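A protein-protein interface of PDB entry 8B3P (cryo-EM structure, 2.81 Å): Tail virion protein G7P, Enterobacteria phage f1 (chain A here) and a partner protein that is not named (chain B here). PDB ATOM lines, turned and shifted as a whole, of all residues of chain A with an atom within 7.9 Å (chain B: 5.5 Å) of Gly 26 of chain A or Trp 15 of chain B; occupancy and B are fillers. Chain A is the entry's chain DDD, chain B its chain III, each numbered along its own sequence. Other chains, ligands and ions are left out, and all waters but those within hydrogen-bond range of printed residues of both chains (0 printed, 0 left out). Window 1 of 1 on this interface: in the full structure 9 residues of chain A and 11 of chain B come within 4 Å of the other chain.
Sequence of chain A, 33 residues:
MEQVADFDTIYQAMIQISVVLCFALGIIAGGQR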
ATOM      1  N   VAL A  20      36.738  14.562  21.821  1.00  0.00           N
ATOM      2  CA  VAL A  20      36.293  14.528  20.432  1.00  0.00           C
ATOM      3  C   VAL A  20      35.661  13.172  20.101  1.00  0.00           C
ATOM      4  O   VAL A  20      34.661  13.138  19.384  1.00  0.00           O
ATOM      5  CB  VAL A  20      37.411  14.915  19.439  1.00  0.00           C
ATOM      6  CG1 VAL A  20      36.937  14.905  17.990  1.00  0.00           C
ATOM      7  CG2 VAL A  20      38.024  16.266  19.776  1.00  0.00           C
ATOM      8  N   LEU A  21      36.225  12.072  20.627  1.00  0.00           N
ATOM      9  CA  LEU A  21      35.739  10.741  20.279  1.00  0.00           C
ATOM     10  C   LEU A  21      34.360  10.475  20.885  1.00  0.00           C
ATOM     11  O   LEU A  21      33.581   9.716  20.308  1.00  0.00           O
ATOM     12  CB  LEU A  21      36.738   9.651  20.690  1.00  0.00           C
ATOM     13  CG  LEU A  21      37.927   9.390  19.759  1.00  0.00           C
ATOM     14  CD1 LEU A  21      38.735   8.201  20.254  1.00  0.00           C
ATOM     15  CD2 LEU A  21      37.499   9.165  18.318  1.00  0.00           C
ATOM     16  N   CYS A  22      34.058  11.108  22.028  1.00  0.00           N
ATOM     17  CA  CYS A  22      32.774  10.903  22.686  1.00  0.00           C
ATOM     18  C   CYS A  22      31.692  11.787  22.068  1.00  0.00           C
ATOM     19  O   CYS A  22      30.506  11.495  22.214  1.00  0.00           O
ATOM     20  CB  CYS A  22      32.869  11.134  24.188  1.00  0.00           C
ATOM     21  SG  CYS A  22      34.066  10.035  24.985  1.00  0.00           S
ATOM     22  N   PHE A  23      32.115  12.865  21.393  1.00  0.00           N
ATOM     23  CA  PHE A  23      31.220  13.731  20.641  1.00  0.00           C
ATOM     24  C   PHE A  23      30.709  12.995  19.400  1.00  0.00           C
ATOM     25  O   PHE A  23      29.514  13.032  19.111  1.00  0.00           O
ATOM     26  CB  PHE A  23      31.897  15.067  20.310  1.00  0.00           C
ATOM     27  CG  PHE A  23      31.008  16.035  19.570  1.00  0.00           C
ATOM     28  CD1 PHE A  23      30.081  16.813  20.251  1.00  0.00           C
ATOM     29  CD2 PHE A  23      31.075  16.147  18.185  1.00  0.00           C
ATOM     30  CE1 PHE A  23      29.248  17.690  19.566  1.00  0.00           C
ATOM     31  CE2 PHE A  23      30.239  17.019  17.499  1.00  0.00           C
ATOM     32  CZ  PHE A  23      29.330  17.792  18.192  1.00  0.00           C
ATOM     33  N   ALA A  24      31.630  12.324  18.690  1.00  0.00           N
ATOM     34  CA  ALA A  24      31.358  11.653  17.427  1.00  0.00           C
ATOM     35  C   ALA A  24      30.403  10.474  17.631  1.00  0.00           C
ATOM     36  O   ALA A  24      29.495  10.262  16.824  1.00  0.00           O
ATOM     37  CB  ALA A  24      32.655  11.225  16.787  1.00  0.00           C
ATOM     38  N   LEU A  25      30.607   9.728  18.726  1.00  0.00           N
ATOM     39  CA  LEU A  25      29.737   8.620  19.092  1.00  0.00           C
ATOM     40  C   LEU A  25      28.355   9.128  19.502  1.00  0.00           C
ATOM     41  O   LEU A  25      27.356   8.461  19.246  1.00  0.00           O
ATOM     42  CB  LEU A  25      30.390   7.808  20.214  1.00  0.00           C
ATOM     43  CG  LEU A  25      31.655   7.043  19.833  1.00  0.00           C
ATOM     44  CD1 LEU A  25      32.326   6.487  21.071  1.00  0.00           C
ATOM     45  CD2 LEU A  25      31.354   5.921  18.849  1.00  0.00           C
ATOM     46  N   GLY A  26      28.313  10.299  20.153  1.00  0.00           N
ATOM     47  CA  GLY A  26      27.068  10.985  20.465  1.00  0.00           C
ATOM     48  C   GLY A  26      26.261  11.312  19.211  1.00  0.00           C
ATOM     49  O   GLY A  26      25.056  11.064  19.179  1.00  0.00           O
ATOM     50  N   ILE A  27      26.948  11.861  18.195  1.00  0.00           N
ATOM     51  CA  ILE A  27      26.339  12.271  16.935  1.00  0.00           C
ATOM     52  C   ILE A  27      25.729  11.053  16.243  1.00  0.00           C
ATOM     53  O   ILE A  27      24.636  11.156  15.690  1.00  0.00           O
ATOM     54  CB  ILE A  27      27.335  13.021  16.016  1.00  0.00           C
ATOM     55  CG1 ILE A  27      27.755  14.392  16.566  1.00  0.00           C
ATOM     56  CG2 ILE A  27      26.826  13.108  14.578  1.00  0.00           C
ATOM     57  CD1 ILE A  27      26.846  15.560  16.210  1.00  0.00           C
ATOM     58  N   ILE A  28      26.435   9.916  16.288  1.00  0.00           N
ATOM     59  CA  ILE A  28      26.008   8.713  15.591  1.00  0.00           C
ATOM     60  C   ILE A  28      24.758   8.156  16.273  1.00  0.00           C
ATOM     61  O   ILE A  28      23.841   7.693  15.598  1.00  0.00           O
ATOM     62  CB  ILE A  28      27.159   7.691  15.493  1.00  0.00           C
ATOM     63  CG1 ILE A  28      28.259   8.187  14.547  1.00  0.00           C
ATOM     64  CG2 ILE A  28      26.660   6.299  15.110  1.00  0.00           C
ATOM     65  CD1 ILE A  28      29.564   7.417  14.634  1.00  0.00           C
ATOM     66  N   ALA A  29      24.731   8.255  17.610  1.00  0.00           N
ATOM     67  CA  ALA A  29      23.658   7.741  18.446  1.00  0.00           C
ATOM     68  C   ALA A  29      22.368   8.505  18.162  1.00  0.00           C
ATOM     69  O   ALA A  29      21.276   7.941  18.263  1.00  0.00           O
ATOM     70  CB  ALA A  29      24.049   7.866  19.897  1.00  0.00           C
ATOM     71  N   GLY A  30      22.540   9.782  17.784  1.00  0.00           N
ATOM     72  CA  GLY A  30      21.476  10.763  17.651  1.00  0.00           C
ATOM     73  C   GLY A  30      20.690  10.622  16.351  1.00  0.00           C
ATOM     74  O   GLY A  30      19.501  10.939  16.321  1.00  0.00           O
ATOM     75  N   GLY A  31      21.368  10.144  15.298  1.00  0.00           N
ATOM     76  CA  GLY A  31      20.783   9.988  13.978  1.00  0.00           C
ATOM     77  C   GLY A  31      20.144   8.616  13.771  1.00  0.00           C
ATOM     78  O   GLY A  31      19.674   8.328  12.670  1.00  0.00           O
ATOM     79  N   GLN A  32      20.169   7.777  14.817  1.00  0.00           N
ATOM     80  CA  GLN A  32      19.464   6.504  14.825  1.00  0.00           C
ATOM     81  C   GLN A  32      17.971   6.775  14.988  1.00  0.00           C
ATOM     82  O   GLN A  32      17.558   7.367  15.984  1.00  0.00           O
ATOM     83  CB  GLN A  32      20.016   5.595  15.924  1.00  0.00           C
ATOM     84  CG  GLN A  32      21.270   4.841  15.492  1.00  0.00           C
ATOM     85  CD  GLN A  32      21.736   3.735  16.410  1.00  0.00           C
ATOM     86  OE1 GLN A  32      22.745   3.845  17.109  1.00  0.00           O
ATOM     87  NE2 GLN A  32      21.022   2.624  16.380  1.00  0.00           N
ATOM     88  N   PHE B  11      29.455  13.506  25.253  1.00  0.00           N
ATOM     89  CA  PHE B  11      28.605  12.556  24.548  1.00  0.00           C
ATOM     90  C   PHE B  11      27.174  13.091  24.455  1.00  0.00           C
ATOM     91  O   PHE B  11      26.552  13.008  23.399  1.00  0.00           O
ATOM     92  CB  PHE B  11      28.700  11.155  25.163  1.00  0.00           C
ATOM     93  CG  PHE B  11      27.688  10.155  24.654  1.00  0.00           C
ATOM     94  CD1 PHE B  11      27.938   9.404  23.511  1.00  0.00           C
ATOM     95  CD2 PHE B  11      26.482   9.958  25.320  1.00  0.00           C
ATOM     96  CE1 PHE B  11      27.000   8.489  23.041  1.00  0.00           C
ATOM     97  CE2 PHE B  11      25.546   9.042  24.852  1.00  0.00           C
ATOM     98  CZ  PHE B  11      25.806   8.309  23.712  1.00  0.00           C
ATOM     99  N   VAL B  12      26.673  13.651  25.563  1.00  0.00           N
ATOM    100  CA  VAL B  12      25.298  14.117  25.667  1.00  0.00           C
ATOM    101  C   VAL B  12      25.100  15.372  24.809  1.00  0.00           C
ATOM    102  O   VAL B  12      23.987  15.630  24.357  1.00  0.00           O
ATOM    103  CB  VAL B  12      24.881  14.307  27.142  1.00  0.00           C
ATOM    104  CG1 VAL B  12      23.484  14.893  27.306  1.00  0.00           C
ATOM    105  CG2 VAL B  12      24.989  13.005  27.924  1.00  0.00           C
ATOM    106  N   LEU B  13      26.178  16.132  24.562  1.00  0.00           N
ATOM    107  CA  LEU B  13      26.090  17.339  23.750  1.00  0.00           C
ATOM    108  C   LEU B  13      25.859  16.963  22.287  1.00  0.00           C
ATOM    109  O   LEU B  13      25.062  17.607  21.605  1.00  0.00           O
ATOM    110  CB  LEU B  13      27.358  18.183  23.935  1.00  0.00           C
ATOM    111  CG  LEU B  13      27.388  19.537  23.220  1.00  0.00           C
ATOM    112  CD1 LEU B  13      26.643  20.601  24.015  1.00  0.00           C
ATOM    113  CD2 LEU B  13      28.823  19.976  22.964  1.00  0.00           C
ATOM    114  N   GLY B  14      26.546  15.905  21.835  1.00  0.00           N
ATOM    115  CA  GLY B  14      26.472  15.417  20.468  1.00  0.00           C
ATOM    116  C   GLY B  14      25.148  14.717  20.170  1.00  0.00           C
ATOM    117  O   GLY B  14      24.668  14.782  19.038  1.00  0.00           O
ATOM    118  N   TRP B  15      24.584  14.046  21.190  1.00  0.00           N
ATOM    119  CA  TRP B  15      23.298  13.364  21.088  1.00  0.00           C
ATOM    120  C   TRP B  15      22.170  14.378  20.885  1.00  0.00           C
ATOM    121  O   TRP B  15      21.268  14.143  20.083  1.00  0.00           O
ATOM    122  CB  TRP B  15      23.050  12.415  22.278  1.00  0.00           C
ATOM    123  CG  TRP B  15      21.725  11.705  22.241  1.00  0.00           C
ATOM    124  CD1 TRP B  15      21.420  10.554  21.570  1.00  0.00           C
ATOM    125  CD2 TRP B  15      20.511  12.113  22.900  1.00  0.00           C
ATOM    126  NE1 TRP B  15      20.104  10.221  21.759  1.00  0.00           N
ATOM    127  CE2 TRP B  15      19.518  11.161  22.566  1.00  0.00           C
ATOM    128  CE3 TRP B  15      20.160  13.187  23.733  1.00  0.00           C
ATOM    129  CZ2 TRP B  15      18.208  11.261  23.041  1.00  0.00           C
ATOM    130  CZ3 TRP B  15      18.865  13.290  24.191  1.00  0.00           C
ATOM    131  CH2 TRP B  15      17.904  12.334  23.853  1.00  0.00           C
ATOM    132  N   CYS B  16      22.258  15.522  21.575  1.00  0.00           N
ATOM    133  CA  CYS B  16      21.204  16.527  21.577  1.00  0.00           C
ATOM    134  C   CYS B  16      21.165  17.302  20.264  1.00  0.00           C
ATOM    135  O   CYS B  16      20.083  17.569  19.742  1.00  0.00           O
ATOM    136  CB  CYS B  16      21.406  17.510  22.722  1.00  0.00           C
ATOM    137  SG  CYS B  16      20.818  16.861  24.307  1.00  0.00           S
ATOM    138  N   LEU B  17      22.352  17.676  19.765  1.00  0.00           N
ATOM    139  CA  LEU B  17      22.501  18.562  18.622  1.00  0.00           C
ATOM    140  C   LEU B  17      21.996  17.886  17.347  1.00  0.00           C
ATOM    141  O   LEU B  17      21.354  18.537  16.522  1.00  0.00           O
ATOM    142  CB  LEU B  17      23.968  18.996  18.500  1.00  0.00           C
ATOM    143  CG  LEU B  17      24.481  19.970  19.566  1.00  0.00           C
ATOM    144  CD1 LEU B  17      25.955  20.283  19.358  1.00  0.00           C
ATOM    145  CD2 LEU B  17      23.664  21.255  19.602  1.00  0.00           C
ATOM    146  N   ARG B  18      22.275  16.580  17.219  1.00  0.00           N
ATOM    147  CA  ARG B  18      21.919  15.803  16.041  1.00  0.00           C
ATOM    148  C   ARG B  18      20.438  15.428  16.055  1.00  0.00           C
ATOM    149  O   ARG B  18      19.784  15.531  15.019  1.00  0.00           O
ATOM    150  CB  ARG B  18      22.809  14.565  15.883  1.00  0.00           C
ATOM    151  CG  ARG B  18      22.468  13.678  14.690  1.00  0.00           C
ATOM    152  CD  ARG B  18      22.689  14.277  13.309  1.00  0.00           C
ATOM    153  NE  ARG B  18      22.374  13.358  12.217  1.00  0.00           N
ATOM    154  CZ  ARG B  18      21.173  13.182  11.663  1.00  0.00           C
ATOM    155  NH1 ARG B  18      20.120  13.859  12.094  1.00  0.00           N
ATOM    156  NH2 ARG B  18      21.021  12.314  10.678  1.00  0.00           N
ATOM    157  N   SER B  19      19.928  14.988  17.216  1.00  0.00           N
ATOM    158  CA  SER B  19      18.564  14.488  17.334  1.00  0.00           C
ATOM    159  C   SER B  19      17.548  15.576  16.994  1.00  0.00           C
ATOM    160  O   SER B  19      16.464  15.257  16.503  1.00  0.00           O
ATOM    161  CB  SER B  19      18.302  13.880  18.680  1.00  0.00           C
ATOM    162  OG  SER B  19      18.651  14.792  19.705  1.00  0.00           O
ATOM    163  N   GLY B  20      17.926  16.842  17.246  1.00  0.00           N
ATOM    164  CA  GLY B  20      17.222  18.027  16.778  1.00  0.00           C
ATOM    165  C   GLY B  20      16.828  17.917  15.307  1.00  0.00           C
ATOM    166  O   GLY B  20      15.668  18.132  14.964  1.00  0.00           O
ATOM    167  N   TYR B  23      14.338  15.031  14.373  1.00  0.00           N
ATOM    168  CA  TYR B  23      12.949  15.341  14.669  1.00  0.00           C
ATOM    169  C   TYR B  23      12.349  16.212  13.568  1.00  0.00           C
ATOM    170  O   TYR B  23      11.215  15.972  13.162  1.00  0.00           O
ATOM    171  CB  TYR B  23      12.790  15.887  16.092  1.00  0.00           C
ATOM    172  CG  TYR B  23      13.255  14.953  17.185  1.00  0.00           C
ATOM    173  CD1 TYR B  23      13.212  13.571  17.028  1.00  0.00           C
ATOM    174  CD2 TYR B  23      13.724  15.448  18.394  1.00  0.00           C
ATOM    175  CE1 TYR B  23      13.643  12.709  18.027  1.00  0.00           C
ATOM    176  CE2 TYR B  23      14.160  14.600  19.404  1.00  0.00           C
ATOM    177  CZ  TYR B  23      14.116  13.227  19.223  1.00  0.00           C
ATOM    178  OH  TYR B  23      14.537  12.391  20.218  1.00  0.00           O
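O of Trp 15 of chain B lies within hydrogen-bond range of OG of Ser 19 of chain B, 2.7 Å away. The backbone carbonyl oxygen of Cys 16 of chain B lies within hydrogen-bond range of the side-chain hydroxyl of Ser 19 of chain B (3.1 Å).
Among the printed residues, pairs that only touch across the chains: Cys 22 of chain A with Phe 11 of chain B, Gly 26 of chain A with Trp 15 of chain B, Ile 27 of chain A with Arg 18 of chain B, Gly 26 of chain A with Phe 11 of chain B, Ile 27 of chain A with Gly 14 of chain B, Phe 23 of chain A with Gly 14 of chain B, Gly 26 of chain A with Gly 14 of chain B, Gly 31 of chain A with Arg 18 of chain B, Gly 30 of chain A with Ser 19 of chain B, Leu 25 of chain A with Phe 11 of chain B, Gly 30 of chain A with Arg 18 of chain B and Gly 30 of chain A with Trp 15 of chain B.
Of the printed residues of chain B, Phe 23 of chain A touches Gly 14 (3.7 Å). Of the printed residues of chain B, Leu 25 of chain A touches Phe 11. Gly 26 of chain A touches just these residues of chain B: Phe 11, Gly 14 and Trp 15. Printed residues of chain B within 4 Å of Gly 30 of chain A: Trp 15, Arg 18 and Ser 19. Printed residues of chain A within 4 Å of Phe 11 of chain B: Cys 22, Leu 25 and Gly 26. Printed residues of chain A within 4 Å of Gly 14 of chain B: Phe 23, Gly 26 and Ile 27. Trp 15 of chain B touches just these residues of chain A: Gly 26 (3.5 Å) and Gly 30 (3.9 Å). No residue of chain A comes within 4 Å of Cys 16 of chain B. The nearest residue of chain B that does not touch Gly 26 of chain A is Arg 18 of chain B (5.3 Å).
Printed residues of chain A that touch a printed residue of chain B: Cys 22, Phe 23, Leu 25, Gly 26, Ile 27, Gly 30 and Gly 31. Among the printed residues, 12 pairs touch across the chains.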
